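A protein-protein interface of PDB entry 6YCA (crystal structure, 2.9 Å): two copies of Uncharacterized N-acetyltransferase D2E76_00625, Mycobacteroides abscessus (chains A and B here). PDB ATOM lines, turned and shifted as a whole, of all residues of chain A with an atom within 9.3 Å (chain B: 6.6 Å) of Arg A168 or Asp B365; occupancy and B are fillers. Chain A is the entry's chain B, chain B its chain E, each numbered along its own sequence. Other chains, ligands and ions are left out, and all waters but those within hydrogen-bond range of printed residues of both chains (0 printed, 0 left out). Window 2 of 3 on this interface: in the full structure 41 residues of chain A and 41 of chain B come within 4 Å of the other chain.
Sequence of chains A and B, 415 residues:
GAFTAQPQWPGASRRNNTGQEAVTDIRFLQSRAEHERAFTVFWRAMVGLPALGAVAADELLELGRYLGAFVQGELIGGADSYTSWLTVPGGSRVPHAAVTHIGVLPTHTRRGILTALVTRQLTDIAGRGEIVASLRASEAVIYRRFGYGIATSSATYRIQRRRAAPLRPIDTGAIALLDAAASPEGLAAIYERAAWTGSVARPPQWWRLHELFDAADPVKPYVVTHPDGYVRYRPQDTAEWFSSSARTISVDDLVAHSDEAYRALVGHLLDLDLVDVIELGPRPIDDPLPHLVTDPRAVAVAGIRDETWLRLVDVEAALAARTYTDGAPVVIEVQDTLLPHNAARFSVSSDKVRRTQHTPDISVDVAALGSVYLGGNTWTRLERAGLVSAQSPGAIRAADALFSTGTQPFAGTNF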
ATOM      1  N   ALA A 164      30.356  -0.002  -7.090  1.00  0.00           N
ATOM      2  CA  ALA A 164      29.447  -0.881  -6.355  1.00  0.00           C
ATOM      3  C   ALA A 164      28.459  -1.560  -7.300  1.00  0.00           C
ATOM      4  O   ALA A 164      27.242  -1.416  -7.192  1.00  0.00           O
ATOM      5  CB  ALA A 164      28.728  -0.104  -5.258  1.00  0.00           C
ATOM      6  N   ALA A 165      29.000  -2.317  -8.224  1.00  0.00           N
ATOM      7  CA  ALA A 165      28.119  -3.163  -9.008  1.00  0.00           C
ATOM      8  C   ALA A 165      27.806  -4.423  -8.204  1.00  0.00           C
ATOM      9  O   ALA A 165      28.677  -4.945  -7.503  1.00  0.00           O
ATOM     10  CB  ALA A 165      28.779  -3.546 -10.327  1.00  0.00           C
ATOM     11  N   PRO A 166      26.571  -4.907  -8.256  1.00  0.00           N
ATOM     12  CA  PRO A 166      26.188  -6.038  -7.402  1.00  0.00           C
ATOM     13  C   PRO A 166      26.919  -7.322  -7.766  1.00  0.00           C
ATOM     14  O   PRO A 166      27.161  -7.615  -8.940  1.00  0.00           O
ATOM     15  CB  PRO A 166      24.679  -6.165  -7.637  1.00  0.00           C
ATOM     16  CG  PRO A 166      24.452  -5.527  -8.966  1.00  0.00           C
ATOM     17  CD  PRO A 166      25.448  -4.415  -9.069  1.00  0.00           C
ATOM     18  N   LEU A 167      27.292  -8.078  -6.730  1.00  0.00           N
ATOM     19  CA  LEU A 167      27.912  -9.383  -6.930  1.00  0.00           C
ATOM     20  C   LEU A 167      26.930 -10.356  -7.568  1.00  0.00           C
ATOM     21  O   LEU A 167      27.275 -11.088  -8.502  1.00  0.00           O
ATOM     22  CB  LEU A 167      28.406  -9.925  -5.589  1.00  0.00           C
ATOM     23  CG  LEU A 167      29.158 -11.257  -5.606  1.00  0.00           C
ATOM     24  CD1 LEU A 167      30.389 -11.161  -6.487  1.00  0.00           C
ATOM     25  CD2 LEU A 167      29.537 -11.686  -4.195  1.00  0.00           C
ATOM     26  N   ARG A 168      25.702 -10.392  -7.058  1.00  0.00           N
ATOM     27  CA  ARG A 168      24.609 -11.160  -7.621  1.00  0.00           C
ATOM     28  C   ARG A 168      23.534 -10.191  -8.094  1.00  0.00           C
ATOM     29  O   ARG A 168      23.436  -9.077  -7.570  1.00  0.00           O
ATOM     30  CB  ARG A 168      24.017 -12.084  -6.548  1.00  0.00           C
ATOM     31  CG  ARG A 168      25.038 -13.034  -5.906  1.00  0.00           C
ATOM     32  CD  ARG A 168      25.312 -14.229  -6.793  1.00  0.00           C
ATOM     33  NE  ARG A 168      26.256 -15.169  -6.195  1.00  0.00           N
ATOM     34  CZ  ARG A 168      27.546 -15.226  -6.511  1.00  0.00           C
ATOM     35  NH1 ARG A 168      28.035 -14.395  -7.422  1.00  0.00           N
ATOM     36  NH2 ARG A 168      28.346 -16.115  -5.928  1.00  0.00           N
ATOM     37  N   PRO A 169      22.731 -10.566  -9.091  1.00  0.00           N
ATOM     38  CA  PRO A 169      21.677  -9.658  -9.569  1.00  0.00           C
ATOM     39  C   PRO A 169      20.684  -9.331  -8.460  1.00  0.00           C
ATOM     40  O   PRO A 169      20.311 -10.195  -7.664  1.00  0.00           O
ATOM     41  CB  PRO A 169      21.012 -10.451 -10.700  1.00  0.00           C
ATOM     42  CG  PRO A 169      22.054 -11.434 -11.139  1.00  0.00           C
ATOM     43  CD  PRO A 169      22.815 -11.795  -9.898  1.00  0.00           C
ATOM     44  N   ILE A 170      20.264  -8.068  -8.405  1.00  0.00           N
ATOM     45  CA  ILE A 170      19.356  -7.584  -7.369  1.00  0.00           C
ATOM     46  C   ILE A 170      18.035  -7.182  -8.014  1.00  0.00           C
ATOM     47  O   ILE A 170      17.998  -6.289  -8.871  1.00  0.00           O
ATOM     48  CB  ILE A 170      19.961  -6.396  -6.615  1.00  0.00           C
ATOM     49  CG1 ILE A 170      21.229  -6.823  -5.878  1.00  0.00           C
ATOM     50  CG2 ILE A 170      18.941  -5.823  -5.662  1.00  0.00           C
ATOM     51  CD1 ILE A 170      21.903  -5.691  -5.122  1.00  0.00           C
ATOM     52  N   ASP A 171      16.945  -7.796  -7.555  1.00  0.00           N
ATOM     53  CA  ASP A 171      15.615  -7.542  -8.100  1.00  0.00           C
ATOM     54  C   ASP A 171      15.031  -6.266  -7.500  1.00  0.00           C
ATOM     55  O   ASP A 171      14.778  -6.198  -6.293  1.00  0.00           O
ATOM     56  CB  ASP A 171      14.705  -8.728  -7.798  1.00  0.00           C
ATOM     57  CG  ASP A 171      13.406  -8.671  -8.563  1.00  0.00           C
ATOM     58  OD1 ASP A 171      13.338  -7.922  -9.559  1.00  0.00           O
ATOM     59  OD2 ASP A 171      12.452  -9.371  -8.163  1.00  0.00           O
ATOM     60  N   ARG A 263      17.933  -6.203  -0.059  1.00  0.00           N
ATOM     61  CA  ARG A 263      18.702  -6.120  -1.295  1.00  0.00           C
ATOM     62  C   ARG A 263      18.067  -5.148  -2.285  1.00  0.00           C
ATOM     63  O   ARG A 263      18.772  -4.358  -2.923  1.00  0.00           O
ATOM     64  CB  ARG A 263      18.858  -7.512  -1.908  1.00  0.00           C
ATOM     65  CG  ARG A 263      19.706  -8.454  -1.067  1.00  0.00           C
ATOM     66  CD  ARG A 263      19.944  -9.782  -1.765  1.00  0.00           C
ATOM     67  NE  ARG A 263      18.714 -10.548  -1.953  1.00  0.00           N
ATOM     68  CZ  ARG A 263      18.300 -11.514  -1.137  1.00  0.00           C
ATOM     69  NH1 ARG A 263      19.021 -11.841  -0.073  1.00  0.00           N
ATOM     70  NH2 ARG A 263      17.168 -12.162  -1.389  1.00  0.00           N
ATOM     71  N   GLY A 267      19.882  -2.089  -3.548  1.00  0.00           N
ATOM     72  CA  GLY A 267      20.050  -2.117  -4.991  1.00  0.00           C
ATOM     73  C   GLY A 267      19.488  -0.885  -5.672  1.00  0.00           C
ATOM     74  O   GLY A 267      20.041  -0.413  -6.671  1.00  0.00           O
ATOM     75  N   LEU A 270      22.271   1.654  -5.245  1.00  0.00           N
ATOM     76  CA  LEU A 270      23.437   1.385  -6.082  1.00  0.00           C
ATOM     77  C   LEU A 270      23.189   1.710  -7.555  1.00  0.00           C
ATOM     78  O   LEU A 270      24.154   1.866  -8.312  1.00  0.00           O
ATOM     79  CB  LEU A 270      23.889  -0.070  -5.908  1.00  0.00           C
ATOM     80  CG  LEU A 270      24.222  -0.578  -4.494  1.00  0.00           C
ATOM     81  CD1 LEU A 270      24.592  -2.052  -4.515  1.00  0.00           C
ATOM     82  CD2 LEU A 270      25.343   0.217  -3.841  1.00  0.00           C
ATOM     83  N   HIS A 291      29.393  -7.486   1.238  1.00  0.00           N
ATOM     84  CA  HIS A 291      29.091  -8.746   0.569  1.00  0.00           C
ATOM     85  C   HIS A 291      28.085  -8.613  -0.567  1.00  0.00           C
ATOM     86  O   HIS A 291      27.855  -9.595  -1.283  1.00  0.00           O
ATOM     87  CB  HIS A 291      28.602  -9.793   1.571  1.00  0.00           C
ATOM     88  CG  HIS A 291      29.626 -10.174   2.591  1.00  0.00           C
ATOM     89  ND1 HIS A 291      30.693 -10.995   2.300  1.00  0.00           N
ATOM     90  CD2 HIS A 291      29.738  -9.861   3.904  1.00  0.00           C
ATOM     91  CE1 HIS A 291      31.425 -11.165   3.386  1.00  0.00           C
ATOM     92  NE2 HIS A 291      30.867 -10.488   4.374  1.00  0.00           N
ATOM     93  N   LEU A 292      27.497  -7.434  -0.767  1.00  0.00           N
ATOM     94  CA  LEU A 292      26.554  -7.249  -1.862  1.00  0.00           C
ATOM     95  C   LEU A 292      27.230  -6.863  -3.166  1.00  0.00           C
ATOM     96  O   LEU A 292      26.606  -6.971  -4.226  1.00  0.00           O
ATOM     97  CB  LEU A 292      25.531  -6.161  -1.525  1.00  0.00           C
ATOM     98  CG  LEU A 292      24.373  -6.505  -0.590  1.00  0.00           C
ATOM     99  CD1 LEU A 292      23.549  -5.258  -0.302  1.00  0.00           C
ATOM    100  CD2 LEU A 292      23.506  -7.608  -1.183  1.00  0.00           C
ATOM    101  N   VAL A 293      28.484  -6.432  -3.118  1.00  0.00           N
ATOM    102  CA  VAL A 293      29.134  -5.830  -4.271  1.00  0.00           C
ATOM    103  C   VAL A 293      30.360  -6.641  -4.662  1.00  0.00           C
ATOM    104  O   VAL A 293      30.985  -7.310  -3.833  1.00  0.00           O
ATOM    105  CB  VAL A 293      29.494  -4.355  -4.003  1.00  0.00           C
ATOM    106  CG1 VAL A 293      28.232  -3.518  -3.961  1.00  0.00           C
ATOM    107  CG2 VAL A 293      30.249  -4.227  -2.697  1.00  0.00           C
ATOM    108  N   THR A 294      30.695  -6.579  -5.953  1.00  0.00           N
ATOM    109  CA  THR A 294      31.882  -7.269  -6.443  1.00  0.00           C
ATOM    110  C   THR A 294      33.153  -6.655  -5.871  1.00  0.00           C
ATOM    111  O   THR A 294      34.170  -7.347  -5.733  1.00  0.00           O
ATOM    112  CB  THR A 294      31.904  -7.217  -7.973  1.00  0.00           C
ATOM    113  OG1 THR A 294      30.646  -7.672  -8.482  1.00  0.00           O
ATOM    114  CG2 THR A 294      33.013  -8.094  -8.533  1.00  0.00           C
ATOM    115  N   ASP A 295      33.107  -5.371  -5.506  1.00  0.00           N
ATOM    116  CA  ASP A 295      34.258  -4.657  -4.964  1.00  0.00           C
ATOM    117  C   ASP A 295      33.960  -4.288  -3.519  1.00  0.00           C
ATOM    118  O   ASP A 295      33.452  -3.191  -3.247  1.00  0.00           O
ATOM    119  CB  ASP A 295      34.528  -3.404  -5.800  1.00  0.00           C
ATOM    120  CG  ASP A 295      35.877  -2.785  -5.505  1.00  0.00           C
ATOM    121  OD1 ASP A 295      36.524  -3.216  -4.527  1.00  0.00           O
ATOM    122  OD2 ASP A 295      36.309  -1.898  -6.278  1.00  0.00           O
ATOM    123  N   ARG B 144      37.855 -13.600  -5.527  1.00  0.00           N
ATOM    124  CA  ARG B 144      36.641 -14.295  -5.113  1.00  0.00           C
ATOM    125  C   ARG B 144      36.173 -15.290  -6.168  1.00  0.00           C
ATOM    126  O   ARG B 144      35.554 -16.306  -5.830  1.00  0.00           O
ATOM    127  CB  ARG B 144      35.528 -13.313  -4.766  1.00  0.00           C
ATOM    128  CG  ARG B 144      34.568 -13.897  -3.751  1.00  0.00           C
ATOM    129  CD  ARG B 144      33.234 -13.203  -3.727  1.00  0.00           C
ATOM    130  NE  ARG B 144      32.346 -13.868  -2.781  1.00  0.00           N
ATOM    131  CZ  ARG B 144      31.634 -14.954  -3.055  1.00  0.00           C
ATOM    132  NH1 ARG B 144      31.696 -15.507  -4.257  1.00  0.00           N
ATOM    133  NH2 ARG B 144      30.856 -15.486  -2.123  1.00  0.00           N
ATOM    134  N   GLY B 147      37.373 -18.831  -5.349  1.00  0.00           N
ATOM    135  CA  GLY B 147      37.022 -19.470  -4.098  1.00  0.00           C
ATOM    136  C   GLY B 147      37.569 -18.806  -2.852  1.00  0.00           C
ATOM    137  O   GLY B 147      37.319 -19.304  -1.745  1.00  0.00           O
ATOM    138  N   GLU B 333      25.853 -27.980   1.825  1.00  0.00           N
ATOM    139  CA  GLU B 333      26.218 -28.309   0.455  1.00  0.00           C
ATOM    140  C   GLU B 333      27.129 -27.204  -0.065  1.00  0.00           C
ATOM    141  O   GLU B 333      26.740 -26.031  -0.088  1.00  0.00           O
ATOM    142  CB  GLU B 333      24.969 -28.424  -0.416  1.00  0.00           C
ATOM    143  CG  GLU B 333      25.268 -28.875  -1.828  1.00  0.00           C
ATOM    144  CD  GLU B 333      24.026 -29.005  -2.681  1.00  0.00           C
ATOM    145  OE1 GLU B 333      22.909 -28.934  -2.133  1.00  0.00           O
ATOM    146  OE2 GLU B 333      24.168 -29.194  -3.905  1.00  0.00           O
ATOM    147  N   VAL B 334      28.347 -27.570  -0.448  1.00  0.00           N
ATOM    148  CA  VAL B 334      29.364 -26.619  -0.876  1.00  0.00           C
ATOM    149  C   VAL B 334      29.543 -26.730  -2.384  1.00  0.00           C
ATOM    150  O   VAL B 334      29.570 -27.835  -2.939  1.00  0.00           O
ATOM    151  CB  VAL B 334      30.690 -26.840  -0.123  1.00  0.00           C
ATOM    152  CG1 VAL B 334      31.720 -25.779  -0.510  1.00  0.00           C
ATOM    153  CG2 VAL B 334      30.452 -26.835   1.381  1.00  0.00           C
ATOM    154  N   GLN B 335      29.641 -25.580  -3.047  1.00  0.00           N
ATOM    155  CA  GLN B 335      29.916 -25.502  -4.475  1.00  0.00           C
ATOM    156  C   GLN B 335      31.368 -25.093  -4.681  1.00  0.00           C
ATOM    157  O   GLN B 335      31.815 -24.079  -4.134  1.00  0.00           O
ATOM    158  CB  GLN B 335      29.015 -24.451  -5.120  1.00  0.00           C
ATOM    159  CG  GLN B 335      29.287 -24.227  -6.594  1.00  0.00           C
ATOM    160  CD  GLN B 335      28.197 -23.418  -7.266  1.00  0.00           C
ATOM    161  OE1 GLN B 335      27.088 -23.293  -6.743  1.00  0.00           O
ATOM    162  NE2 GLN B 335      28.513 -22.845  -8.424  1.00  0.00           N
ATOM    163  N   ASP B 336      32.099 -25.874  -5.476  1.00  0.00           N
ATOM    164  CA  ASP B 336      33.506 -25.592  -5.747  1.00  0.00           C
ATOM    165  C   ASP B 336      33.779 -26.012  -7.185  1.00  0.00           C
ATOM    166  O   ASP B 336      33.759 -27.208  -7.492  1.00  0.00           O
ATOM    167  CB  ASP B 336      34.399 -26.370  -4.785  1.00  0.00           C
ATOM    168  CG  ASP B 336      35.806 -25.805  -4.702  1.00  0.00           C
ATOM    169  OD1 ASP B 336      36.257 -25.169  -5.680  1.00  0.00           O
ATOM    170  OD2 ASP B 336      36.473 -26.011  -3.664  1.00  0.00           O
ATOM    171  N   SER B 363      22.972 -24.394   1.254  1.00  0.00           N
ATOM    172  CA  SER B 363      23.773 -24.505   0.043  1.00  0.00           C
ATOM    173  C   SER B 363      24.546 -23.204  -0.116  1.00  0.00           C
ATOM    174  O   SER B 363      23.964 -22.118  -0.034  1.00  0.00           O
ATOM    175  CB  SER B 363      22.881 -24.760  -1.176  1.00  0.00           C
ATOM    176  OG  SER B 363      23.647 -25.157  -2.301  1.00  0.00           O
ATOM    177  N   VAL B 364      25.855 -23.314  -0.333  1.00  0.00           N
ATOM    178  CA  VAL B 364      26.725 -22.146  -0.379  1.00  0.00           C
ATOM    179  C   VAL B 364      27.950 -22.478  -1.220  1.00  0.00           C
ATOM    180  O   VAL B 364      28.379 -23.633  -1.292  1.00  0.00           O
ATOM    181  CB  VAL B 364      27.099 -21.704   1.060  1.00  0.00           C
ATOM    182  CG1 VAL B 364      28.021 -22.723   1.720  1.00  0.00           C
ATOM    183  CG2 VAL B 364      27.713 -20.325   1.064  1.00  0.00           C
ATOM    184  N   ASP B 365      28.519 -21.457  -1.856  1.00  0.00           N
ATOM    185  CA  ASP B 365      29.782 -21.645  -2.559  1.00  0.00           C
ATOM    186  C   ASP B 365      30.961 -21.600  -1.588  1.00  0.00           C
ATOM    187  O   ASP B 365      30.872 -21.072  -0.476  1.00  0.00           O
ATOM    188  CB  ASP B 365      29.957 -20.615  -3.680  1.00  0.00           C
ATOM    189  CG  ASP B 365      30.059 -19.188  -3.161  1.00  0.00           C
ATOM    190  OD1 ASP B 365      29.472 -18.889  -2.099  1.00  0.00           O
ATOM    191  OD2 ASP B 365      30.731 -18.365  -3.818  1.00  0.00           O
ATOM    192  N   VAL B 366      32.080 -22.184  -2.026  1.00  0.00           N
ATOM    193  CA  VAL B 366      33.240 -22.346  -1.151  1.00  0.00           C
ATOM    194  C   VAL B 366      33.806 -21.002  -0.704  1.00  0.00           C
ATOM    195  O   VAL B 366      34.380 -20.894   0.388  1.00  0.00           O
ATOM    196  CB  VAL B 366      34.299 -23.245  -1.820  1.00  0.00           C
ATOM    197  CG1 VAL B 366      34.908 -22.545  -3.023  1.00  0.00           C
ATOM    198  CG2 VAL B 366      35.373 -23.641  -0.821  1.00  0.00           C
ATOM    199  N   ALA B 367      33.659 -19.960  -1.527  1.00  0.00           N
ATOM    200  CA  ALA B 367      34.165 -18.644  -1.149  1.00  0.00           C
ATOM    201  C   ALA B 367      33.426 -18.108   0.069  1.00  0.00           C
ATOM    202  O   ALA B 367      34.043 -17.598   1.012  1.00  0.00           O
ATOM    203  CB  ALA B 367      34.053 -17.675  -2.324  1.00  0.00           C
ATOM    204  N   ALA B 368      32.096 -18.210   0.068  1.00  0.00           N
ATOM    205  CA  ALA B 368      31.333 -17.723   1.210  1.00  0.00           C
ATOM    206  C   ALA B 368      31.518 -18.618   2.426  1.00  0.00           C
ATOM    207  O   ALA B 368      31.500 -18.128   3.560  1.00  0.00           O
ATOM    208  CB  ALA B 368      29.857 -17.581   0.848  1.00  0.00           C
ATOM    209  N   LEU B 369      31.700 -19.925   2.215  1.00  0.00           N
ATOM    210  CA  LEU B 369      32.008 -20.806   3.336  1.00  0.00           C
ATOM    211  C   LEU B 369      33.326 -20.416   3.987  1.00  0.00           C
ATOM    212  O   LEU B 369      33.462 -20.471   5.215  1.00  0.00           O
ATOM    213  CB  LEU B 369      32.050 -22.263   2.878  1.00  0.00           C
ATOM    214  CG  LEU B 369      32.400 -23.228   4.014  1.00  0.00           C
ATOM    215  CD1 LEU B 369      31.339 -23.156   5.096  1.00  0.00           C
ATOM    216  CD2 LEU B 369      32.569 -24.656   3.514  1.00  0.00           C
ATOM    217  N   GLY B 370      34.308 -20.007   3.181  1.00  0.00           N
ATOM    218  CA  GLY B 370      35.547 -19.513   3.749  1.00  0.00           C
ATOM    219  C   GLY B 370      35.350 -18.272   4.593  1.00  0.00           C
ATOM    220  O   GLY B 370      36.011 -18.104   5.619  1.00  0.00           O
ATOM    221  N   ALA B 385      22.961 -11.014   2.304  1.00  0.00           N
ATOM    222  CA  ALA B 385      23.586 -10.519   1.089  1.00  0.00           C
ATOM    223  C   ALA B 385      23.266 -11.373  -0.126  1.00  0.00           C
ATOM    224  O   ALA B 385      23.662 -11.006  -1.237  1.00  0.00           O
ATOM    225  CB  ALA B 385      25.101 -10.446   1.276  1.00  0.00           C
ATOM    226  N   GLY B 386      22.557 -12.485   0.049  1.00  0.00           N
ATOM    227  CA  GLY B 386      22.205 -13.345  -1.062  1.00  0.00           C
ATOM    228  C   GLY B 386      23.243 -14.377  -1.438  1.00  0.00           C
ATOM    229  O   GLY B 386      23.223 -14.868  -2.571  1.00  0.00           O
ATOM    230  N   LEU B 387      24.149 -14.728  -0.525  1.00  0.00           N
ATOM    231  CA  LEU B 387      25.203 -15.695  -0.793  1.00  0.00           C
ATOM    232  C   LEU B 387      24.954 -17.050  -0.148  1.00  0.00           C
ATOM    233  O   LEU B 387      25.803 -17.940  -0.267  1.00  0.00           O
ATOM    234  CB  LEU B 387      26.556 -15.156  -0.321  1.00  0.00           C
ATOM    235  CG  LEU B 387      27.092 -13.911  -1.016  1.00  0.00           C
ATOM    236  CD1 LEU B 387      28.310 -13.395  -0.290  1.00  0.00           C
ATOM    237  CD2 LEU B 387      27.431 -14.230  -2.454  1.00  0.00           C
ATOM    238  N   VAL B 388      23.826 -17.230   0.535  1.00  0.00           N
ATOM    239  CA  VAL B 388      23.506 -18.484   1.209  1.00  0.00           C
ATOM    240  C   VAL B 388      22.047 -18.822   0.940  1.00  0.00           C
ATOM    241  O   VAL B 388      21.176 -17.953   1.045  1.00  0.00           O
ATOM    242  CB  VAL B 388      23.767 -18.400   2.727  1.00  0.00           C
ATOM    243  CG1 VAL B 388      23.371 -19.699   3.408  1.00  0.00           C
ATOM    244  CG2 VAL B 388      25.228 -18.087   3.000  1.00  0.00           C
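Among the printed residues, merely in contact across the chains: Leu A292 with Ala B385, His A291 with Ala B385, Arg A263 with Gly B386, Leu A167 with Leu B387, Arg A168 with Arg B144, Leu A167 with Arg B144, Arg A263 with Ala B385 and His A291 with Leu B387.
No position is printed for both chains. Of the 9 pairs that touch across the chains among the printed residues, none has its exchanged pair printed and touching as well.
NH2 of Arg A168 lies within salt-bridge range of OD2 of Asp B365.
Of the 16 printed residues of chain A, 5 touch a printed residue of chain B. Of the 18 printed residues of chain B, 5 touch a printed residue of chain A. Among the printed residues, Asp or Glu carboxylates within 4 Å of a Lys or Arg side-chain nitrogen of the other chain: Arg A168 with Asp B365 (3.9 Å).
The backbone NH (N) of Leu A167 sits at hydrogen-bond distance from the backbone carbonyl oxygen (O) of Leu A292 (2.8 Å). The guanidinium group (NH1) of Arg B144 lies within salt-bridge range of the side-chain carboxylate (OD2) of Asp B365 (3.0 Å). The side-chain carboxylate (OD1) of Asp B365 lies close to the backbone NH (N) of Ala B368, at 3.5 Å.
Arg A168 touches two residues of chain B. Of chain A, only Arg A168 (3.9 Å) comes within 4 Å of Asp B365. No residue of chain A comes within 4 Å of Val B364. No residue of chain A comes within 4 Å of Val B366. No residue of chain A comes within 4 Å of Ala B367. No residue of chain A comes within 4 Å of Ala B368. Of the printed residues of chain B, Arg A263 touches Ala B385 and Gly B386. Of the printed residues of chain A, Leu B387 touches Leu A167 (3.7 Å) and His A291 (3.95 Å). Of the printed residues of chain A, Ala B385 touches Arg A263 (3.9 Å), His A291 (3.6 Å) and Leu A292 (3.4 Å). Of the printed residues of chain A, Gly B386 touches Arg A263 (3.6 Å). Of the printed residues of chain B, Leu A292 touches Ala B385. Asp B336 touches none of the printed residues of chain A. The nearest printed residue of chain A that does not touch Ala B385 is Arg A168 (5.3 Å).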
